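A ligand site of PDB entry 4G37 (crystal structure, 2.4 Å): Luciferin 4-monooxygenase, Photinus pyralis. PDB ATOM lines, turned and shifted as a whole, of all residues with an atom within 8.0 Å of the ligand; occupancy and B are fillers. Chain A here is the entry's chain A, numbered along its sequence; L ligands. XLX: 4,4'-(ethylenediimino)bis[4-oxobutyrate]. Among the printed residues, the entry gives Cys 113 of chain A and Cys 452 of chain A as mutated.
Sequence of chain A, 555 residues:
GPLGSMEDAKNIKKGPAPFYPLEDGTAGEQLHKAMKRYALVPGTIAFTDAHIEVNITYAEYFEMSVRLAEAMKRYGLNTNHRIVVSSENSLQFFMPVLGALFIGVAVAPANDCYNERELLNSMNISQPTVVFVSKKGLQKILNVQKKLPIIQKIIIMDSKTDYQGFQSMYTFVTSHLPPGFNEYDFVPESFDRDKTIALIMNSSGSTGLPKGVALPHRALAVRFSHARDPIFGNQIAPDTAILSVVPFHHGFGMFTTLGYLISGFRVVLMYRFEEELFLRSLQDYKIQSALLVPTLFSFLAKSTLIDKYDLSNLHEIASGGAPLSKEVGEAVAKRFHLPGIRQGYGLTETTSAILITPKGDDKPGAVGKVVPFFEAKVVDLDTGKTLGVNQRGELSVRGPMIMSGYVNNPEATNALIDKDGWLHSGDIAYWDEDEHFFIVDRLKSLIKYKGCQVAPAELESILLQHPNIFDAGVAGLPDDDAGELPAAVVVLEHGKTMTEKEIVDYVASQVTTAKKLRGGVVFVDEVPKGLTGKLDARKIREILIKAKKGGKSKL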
ATOM      1  N   GLU A  88      -1.100 -14.542  15.858  1.00  0.00           N
ATOM      2  CA  GLU A  88      -1.488 -14.791  17.237  1.00  0.00           C
ATOM      3  C   GLU A  88      -2.057 -13.494  17.838  1.00  0.00           C
ATOM      4  O   GLU A  88      -1.848 -12.413  17.275  1.00  0.00           O
ATOM      5  CB  GLU A  88      -0.290 -15.280  18.043  1.00  0.00           C
ATOM      6  CG  GLU A  88       0.858 -14.269  18.195  1.00  0.00           C
ATOM      7  CD  GLU A  88       1.757 -14.154  16.955  1.00  0.00           C
ATOM      8  OE1 GLU A  88       1.395 -14.703  15.881  1.00  0.00           O
ATOM      9  OE2 GLU A  88       2.827 -13.511  17.069  1.00  0.00           O
ATOM     10  N   ASN A 111      -6.312 -18.819  11.364  1.00  0.00           N
ATOM     11  CA  ASN A 111      -5.918 -19.352  12.649  1.00  0.00           C
ATOM     12  C   ASN A 111      -4.404 -19.512  12.656  1.00  0.00           C
ATOM     13  O   ASN A 111      -3.839 -20.207  11.807  1.00  0.00           O
ATOM     14  CB  ASN A 111      -6.620 -20.699  12.873  1.00  0.00           C
ATOM     15  CG  ASN A 111      -6.351 -21.290  14.246  1.00  0.00           C
ATOM     16  OD1 ASN A 111      -5.614 -20.710  15.056  1.00  0.00           O
ATOM     17  ND2 ASN A 111      -6.941 -22.442  14.513  1.00  0.00           N
ATOM     18  N   ASP A 112      -3.723 -18.855  13.596  1.00  0.00           N
ATOM     19  CA  ASP A 112      -2.273 -18.953  13.637  1.00  0.00           C
ATOM     20  C   ASP A 112      -1.785 -20.379  13.970  1.00  0.00           C
ATOM     21  O   ASP A 112      -0.599 -20.694  13.789  1.00  0.00           O
ATOM     22  CB  ASP A 112      -1.691 -17.919  14.617  1.00  0.00           C
ATOM     23  CG  ASP A 112      -2.258 -18.069  16.010  1.00  0.00           C
ATOM     24  OD1 ASP A 112      -3.482 -17.849  16.178  1.00  0.00           O
ATOM     25  OD2 ASP A 112      -1.478 -18.409  16.934  1.00  0.00           O
ATOM     26  N   CYS A 113      -2.688 -21.255  14.424  1.00  0.00           N
ATOM     27  CA  CYS A 113      -2.365 -22.668  14.686  1.00  0.00           C
ATOM     28  C   CYS A 113      -2.361 -23.583  13.443  1.00  0.00           C
ATOM     29  O   CYS A 113      -1.755 -24.647  13.455  1.00  0.00           O
ATOM     30  CB  CYS A 113      -3.330 -23.273  15.714  1.00  0.00           C
ATOM     31  SG  CYS A 113      -3.181 -22.595  17.362  1.00  0.00           S
ATOM     32  N   TYR A 114      -3.073 -23.148  12.405  1.00  0.00           N
ATOM     33  CA  TYR A 114      -3.161 -23.866  11.119  1.00  0.00           C
ATOM     34  C   TYR A 114      -1.824 -24.410  10.588  1.00  0.00           C
ATOM     35  O   TYR A 114      -0.807 -23.746  10.651  1.00  0.00           O
ATOM     36  CB  TYR A 114      -3.721 -22.908  10.056  1.00  0.00           C
ATOM     37  CG  TYR A 114      -5.217 -22.864   9.927  1.00  0.00           C
ATOM     38  CD1 TYR A 114      -6.046 -23.544  10.815  1.00  0.00           C
ATOM     39  CD2 TYR A 114      -5.806 -22.148   8.902  1.00  0.00           C
ATOM     40  CE1 TYR A 114      -7.428 -23.501  10.671  1.00  0.00           C
ATOM     41  CE2 TYR A 114      -7.176 -22.098   8.752  1.00  0.00           C
ATOM     42  CZ  TYR A 114      -7.986 -22.777   9.630  1.00  0.00           C
ATOM     43  OH  TYR A 114      -9.356 -22.712   9.445  1.00  0.00           O
ATOM     44  N   LYS A 140       5.090 -20.058   6.746  1.00  0.00           N
ATOM     45  CA  LYS A 140       3.907 -20.763   6.261  1.00  0.00           C
ATOM     46  C   LYS A 140       3.234 -19.978   5.156  1.00  0.00           C
ATOM     47  O   LYS A 140       2.763 -20.537   4.162  1.00  0.00           O
ATOM     48  CB  LYS A 140       2.917 -21.003   7.414  1.00  0.00           C
ATOM     49  CG  LYS A 140       3.508 -21.817   8.551  1.00  0.00           C
ATOM     50  CD  LYS A 140       2.426 -22.311   9.493  1.00  0.00           C
ATOM     51  CE  LYS A 140       3.009 -23.245  10.555  1.00  0.00           C
ATOM     52  NZ  LYS A 140       1.996 -23.678  11.551  1.00  0.00           N
ATOM     53  N   PRO A 247      -9.123 -15.814  21.531  1.00  0.00           N
ATOM     54  CA  PRO A 247      -8.407 -15.694  20.262  1.00  0.00           C
ATOM     55  C   PRO A 247      -9.108 -14.741  19.307  1.00  0.00           C
ATOM     56  O   PRO A 247     -10.324 -14.835  19.087  1.00  0.00           O
ATOM     57  CB  PRO A 247      -8.466 -17.127  19.697  1.00  0.00           C
ATOM     58  CG  PRO A 247      -8.618 -18.002  20.886  1.00  0.00           C
ATOM     59  CD  PRO A 247      -9.445 -17.210  21.872  1.00  0.00           C
ATOM     60  N   HIS A 249      -8.841 -14.558  16.151  1.00  0.00           N
ATOM     61  CA  HIS A 249      -9.105 -15.095  14.811  1.00  0.00           C
ATOM     62  C   HIS A 249     -10.449 -15.812  14.704  1.00  0.00           C
ATOM     63  O   HIS A 249     -10.893 -16.150  13.617  1.00  0.00           O
ATOM     64  CB  HIS A 249      -7.965 -16.003  14.315  1.00  0.00           C
ATOM     65  CG  HIS A 249      -7.679 -17.151  15.229  1.00  0.00           C
ATOM     66  ND1 HIS A 249      -8.502 -18.258  15.291  1.00  0.00           N
ATOM     67  CD2 HIS A 249      -6.685 -17.358  16.120  1.00  0.00           C
ATOM     68  CE1 HIS A 249      -8.023 -19.100  16.193  1.00  0.00           C
ATOM     69  NE2 HIS A 249      -6.913 -18.589  16.705  1.00  0.00           N
ATOM     70  N   TYR A 271      -2.523 -13.562  26.712  1.00  0.00           N
ATOM     71  CA  TYR A 271      -2.367 -14.577  25.684  1.00  0.00           C
ATOM     72  C   TYR A 271      -2.241 -15.945  26.321  1.00  0.00           C
ATOM     73  O   TYR A 271      -2.817 -16.930  25.845  1.00  0.00           O
ATOM     74  CB  TYR A 271      -1.119 -14.294  24.847  1.00  0.00           C
ATOM     75  CG  TYR A 271      -1.001 -12.847  24.398  1.00  0.00           C
ATOM     76  CD1 TYR A 271       0.219 -12.198  24.423  1.00  0.00           C
ATOM     77  CD2 TYR A 271      -2.122 -12.141  23.969  1.00  0.00           C
ATOM     78  CE1 TYR A 271       0.329 -10.879  24.023  1.00  0.00           C
ATOM     79  CE2 TYR A 271      -2.017 -10.822  23.561  1.00  0.00           C
ATOM     80  CZ  TYR A 271      -0.787 -10.186  23.591  1.00  0.00           C
ATOM     81  OH  TYR A 271      -0.685  -8.877  23.185  1.00  0.00           O
ATOM     82  N   LYS A 448     -14.428 -29.538  21.011  1.00  0.00           N
ATOM     83  CA  LYS A 448     -13.671 -28.352  21.357  1.00  0.00           C
ATOM     84  C   LYS A 448     -12.691 -28.684  22.470  1.00  0.00           C
ATOM     85  O   LYS A 448     -13.075 -28.835  23.632  1.00  0.00           O
ATOM     86  CB  LYS A 448     -14.580 -27.208  21.765  1.00  0.00           C
ATOM     87  CG  LYS A 448     -15.376 -26.623  20.622  1.00  0.00           C
ATOM     88  CD  LYS A 448     -15.589 -25.166  20.856  1.00  0.00           C
ATOM     89  CE  LYS A 448     -16.594 -24.603  19.891  1.00  0.00           C
ATOM     90  NZ  LYS A 448     -16.680 -23.135  20.080  1.00  0.00           N
ATOM     91  N   TYR A 449     -11.421 -28.807  22.097  1.00  0.00           N
ATOM     92  CA  TYR A 449     -10.336 -29.049  23.030  1.00  0.00           C
ATOM     93  C   TYR A 449      -9.669 -27.727  23.411  1.00  0.00           C
ATOM     94  O   TYR A 449      -9.036 -27.089  22.558  1.00  0.00           O
ATOM     95  CB  TYR A 449      -9.301 -30.007  22.421  1.00  0.00           C
ATOM     96  CG  TYR A 449      -7.999 -30.056  23.183  1.00  0.00           C
ATOM     97  CD1 TYR A 449      -7.902 -30.748  24.386  1.00  0.00           C
ATOM     98  CD2 TYR A 449      -6.873 -29.379  22.725  1.00  0.00           C
ATOM     99  CE1 TYR A 449      -6.710 -30.790  25.094  1.00  0.00           C
ATOM    100  CE2 TYR A 449      -5.674 -29.416  23.418  1.00  0.00           C
ATOM    101  CZ  TYR A 449      -5.601 -30.122  24.611  1.00  0.00           C
ATOM    102  OH  TYR A 449      -4.403 -30.159  25.304  1.00  0.00           O
ATOM    103  N   LYS A 450      -9.788 -27.337  24.681  1.00  0.00           N
ATOM    104  CA  LYS A 450      -9.295 -26.035  25.143  1.00  0.00           C
ATOM    105  C   LYS A 450      -9.657 -24.930  24.144  1.00  0.00           C
ATOM    106  O   LYS A 450      -8.781 -24.212  23.660  1.00  0.00           O
ATOM    107  CB  LYS A 450      -7.779 -26.060  25.408  1.00  0.00           C
ATOM    108  N   GLY A 451     -10.943 -24.850  23.803  1.00  0.00           N
ATOM    109  CA  GLY A 451     -11.448 -23.866  22.869  1.00  0.00           C
ATOM    110  C   GLY A 451     -11.251 -24.161  21.388  1.00  0.00           C
ATOM    111  O   GLY A 451     -11.955 -23.604  20.560  1.00  0.00           O
ATOM    112  N   CYS A 452     -10.281 -25.012  21.050  1.00  0.00           N
ATOM    113  CA  CYS A 452      -9.929 -25.241  19.646  1.00  0.00           C
ATOM    114  C   CYS A 452     -10.824 -26.305  19.000  1.00  0.00           C
ATOM    115  O   CYS A 452     -11.013 -27.384  19.553  1.00  0.00           O
ATOM    116  CB  CYS A 452      -8.444 -25.621  19.511  1.00  0.00           C
ATOM    117  SG  CYS A 452      -7.232 -24.313  19.877  1.00  0.00           S
ATOM    118  N   GLN A 453     -11.351 -25.996  17.819  1.00  0.00           N
ATOM    119  CA  GLN A 453     -12.236 -26.923  17.122  1.00  0.00           C
ATOM    120  C   GLN A 453     -11.482 -28.136  16.570  1.00  0.00           C
ATOM    121  O   GLN A 453     -10.445 -27.989  15.935  1.00  0.00           O
ATOM    122  CB  GLN A 453     -12.958 -26.225  15.975  1.00  0.00           C
ATOM    123  CG  GLN A 453     -13.826 -25.057  16.417  1.00  0.00           C
ATOM    124  CD  GLN A 453     -14.544 -24.430  15.246  1.00  0.00           C
ATOM    125  OE1 GLN A 453     -15.178 -25.120  14.450  1.00  0.00           O
ATOM    126  NE2 GLN A 453     -14.430 -23.102  15.126  1.00  0.00           N
ATOM    127  N   VAL A 454     -12.025 -29.329  16.824  1.00  0.00           N
ATOM    128  CA  VAL A 454     -11.455 -30.579  16.301  1.00  0.00           C
ATOM    129  C   VAL A 454     -12.486 -31.375  15.511  1.00  0.00           C
ATOM    130  O   VAL A 454     -13.422 -31.938  16.072  1.00  0.00           O
ATOM    131  CB  VAL A 454     -10.891 -31.472  17.430  1.00  0.00           C
ATOM    132  CG1 VAL A 454     -10.605 -32.877  16.921  1.00  0.00           C
ATOM    133  CG2 VAL A 454      -9.629 -30.859  18.031  1.00  0.00           C
ATOM    134  N   THR A 512      -1.355 -32.230  14.130  1.00  0.00           N
ATOM    135  CA  THR A 512      -1.013 -31.049  14.919  1.00  0.00           C
ATOM    136  C   THR A 512      -1.532 -31.197  16.355  1.00  0.00           C
ATOM    137  O   THR A 512      -2.438 -31.994  16.595  1.00  0.00           O
ATOM    138  CB  THR A 512      -1.574 -29.758  14.308  1.00  0.00           C
ATOM    139  OG1 THR A 512      -3.008 -29.845  14.225  1.00  0.00           O
ATOM    140  CG2 THR A 512      -0.973 -29.511  12.919  1.00  0.00           C
ATOM    141  N   THR A 513      -0.959 -30.430  17.272  1.00  0.00           N
ATOM    142  CA  THR A 513      -1.133 -30.688  18.720  1.00  0.00           C
ATOM    143  C   THR A 513      -2.574 -30.682  19.239  1.00  0.00           C
ATOM    144  O   THR A 513      -2.904 -31.438  20.148  1.00  0.00           O
ATOM    145  CB  THR A 513      -0.290 -29.753  19.608  1.00  0.00           C
ATOM    146  OG1 THR A 513      -0.963 -28.496  19.744  1.00  0.00           O
ATOM    147  CG2 THR A 513       1.109 -29.544  19.009  1.00  0.00           C
ATOM    148  N   ALA A 514      -3.427 -29.839  18.669  1.00  0.00           N
ATOM    149  CA  ALA A 514      -4.811 -29.755  19.136  1.00  0.00           C
ATOM    150  C   ALA A 514      -5.613 -31.026  18.825  1.00  0.00           C
ATOM    151  O   ALA A 514      -6.550 -31.373  19.567  1.00  0.00           O
ATOM    152  CB  ALA A 514      -5.493 -28.535  18.543  1.00  0.00           C
ATOM    153  N   LYS A 515      -5.248 -31.733  17.765  1.00  0.00           N
ATOM    154  CA  LYS A 515      -5.990 -32.907  17.344  1.00  0.00           C
ATOM    155  C   LYS A 515      -5.506 -34.214  17.962  1.00  0.00           C
ATOM    156  O   LYS A 515      -6.008 -35.296  17.618  1.00  0.00           O
ATOM    157  CB  LYS A 515      -5.967 -33.052  15.819  1.00  0.00           C
ATOM    158  CG  LYS A 515      -6.663 -31.945  15.064  1.00  0.00           C
ATOM    159  CD  LYS A 515      -5.751 -31.427  13.986  1.00  0.00           C
ATOM    160  CE  LYS A 515      -6.485 -30.556  12.991  1.00  0.00           C
ATOM    161  NZ  LYS A 515      -5.593 -30.296  11.822  1.00  0.00           N
ATOM    162  N   ARG A 518      -6.019 -37.249  22.959  1.00  0.00           N
ATOM    163  CA  ARG A 518      -5.751 -37.224  24.399  1.00  0.00           C
ATOM    164  C   ARG A 518      -6.767 -37.991  25.217  1.00  0.00           C
ATOM    165  O   ARG A 518      -6.478 -38.388  26.342  1.00  0.00           O
ATOM    166  CB  ARG A 518      -5.689 -35.783  24.895  1.00  0.00           C
ATOM    167  CG  ARG A 518      -4.563 -35.006  24.279  1.00  0.00           C
ATOM    168  CD  ARG A 518      -4.308 -33.699  25.001  1.00  0.00           C
ATOM    169  NE  ARG A 518      -3.168 -33.017  24.424  1.00  0.00           N
ATOM    170  CZ  ARG A 518      -3.197 -32.411  23.241  1.00  0.00           C
ATOM    171  NH1 ARG A 518      -4.323 -32.413  22.533  1.00  0.00           N
ATOM    172  NH2 ARG A 518      -2.101 -31.821  22.777  1.00  0.00           N
HETATM  173  O13 XLX L   1      -5.684 -23.381  22.417  1.00  0.00           O
HETATM  174  C12 XLX L   1      -5.175 -24.271  21.744  1.00  0.00           C
HETATM  175  C11 XLX L   1      -6.009 -25.184  20.874  1.00  0.00           C
HETATM  176  N8  XLX L   1      -3.858 -24.464  21.776  1.00  0.00           N
HETATM  177  C7  XLX L   1      -3.197 -25.492  21.002  1.00  0.00           C
HETATM  178  C6  XLX L   1      -2.553 -24.875  19.770  1.00  0.00           C
HETATM  179  N1  XLX L   1      -1.722 -23.733  20.133  1.00  0.00           N
HETATM  180  C2  XLX L   1      -1.184 -22.886  19.240  1.00  0.00           C
HETATM  181  O15 XLX L   1      -0.492 -21.937  19.575  1.00  0.00           O
HETATM  182  C3  XLX L   1      -1.501 -23.144  17.791  1.00  0.00           C
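SG of Cys 452 is bonded to C11 of the ligand, 1.8 Å away. The side-chain sulfur (SG) of Cys 113 is bonded to a carbon (C3) of the ligand, at 1.8 Å.
The guanidinium group (NE) of Arg 518 is in hydrogen-bond range of the side-chain hydroxyl (OH) of Tyr 449 (3.2 Å). O of Thr 513 lies within hydrogen-bond range of NH2 of Arg 518 (2.8 Å). The side-chain amide oxygen of Asn 111 lies close to the backbone NH of Cys 113, 3.0 Å away.
The backbone carbonyl oxygen of Lys 450 lies close to an oxygen (O13) of the ligand, at 3.4 Å. O of Tyr 449 touches C11 of the ligand (3.95 Å). OG1 of Thr 513 touches C7 of the ligand, 3.9 Å away. Five residues have an atom within 4 Å of the ligand: Cys 113, Tyr 449, Lys 450, Cys 452 and Thr 513.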
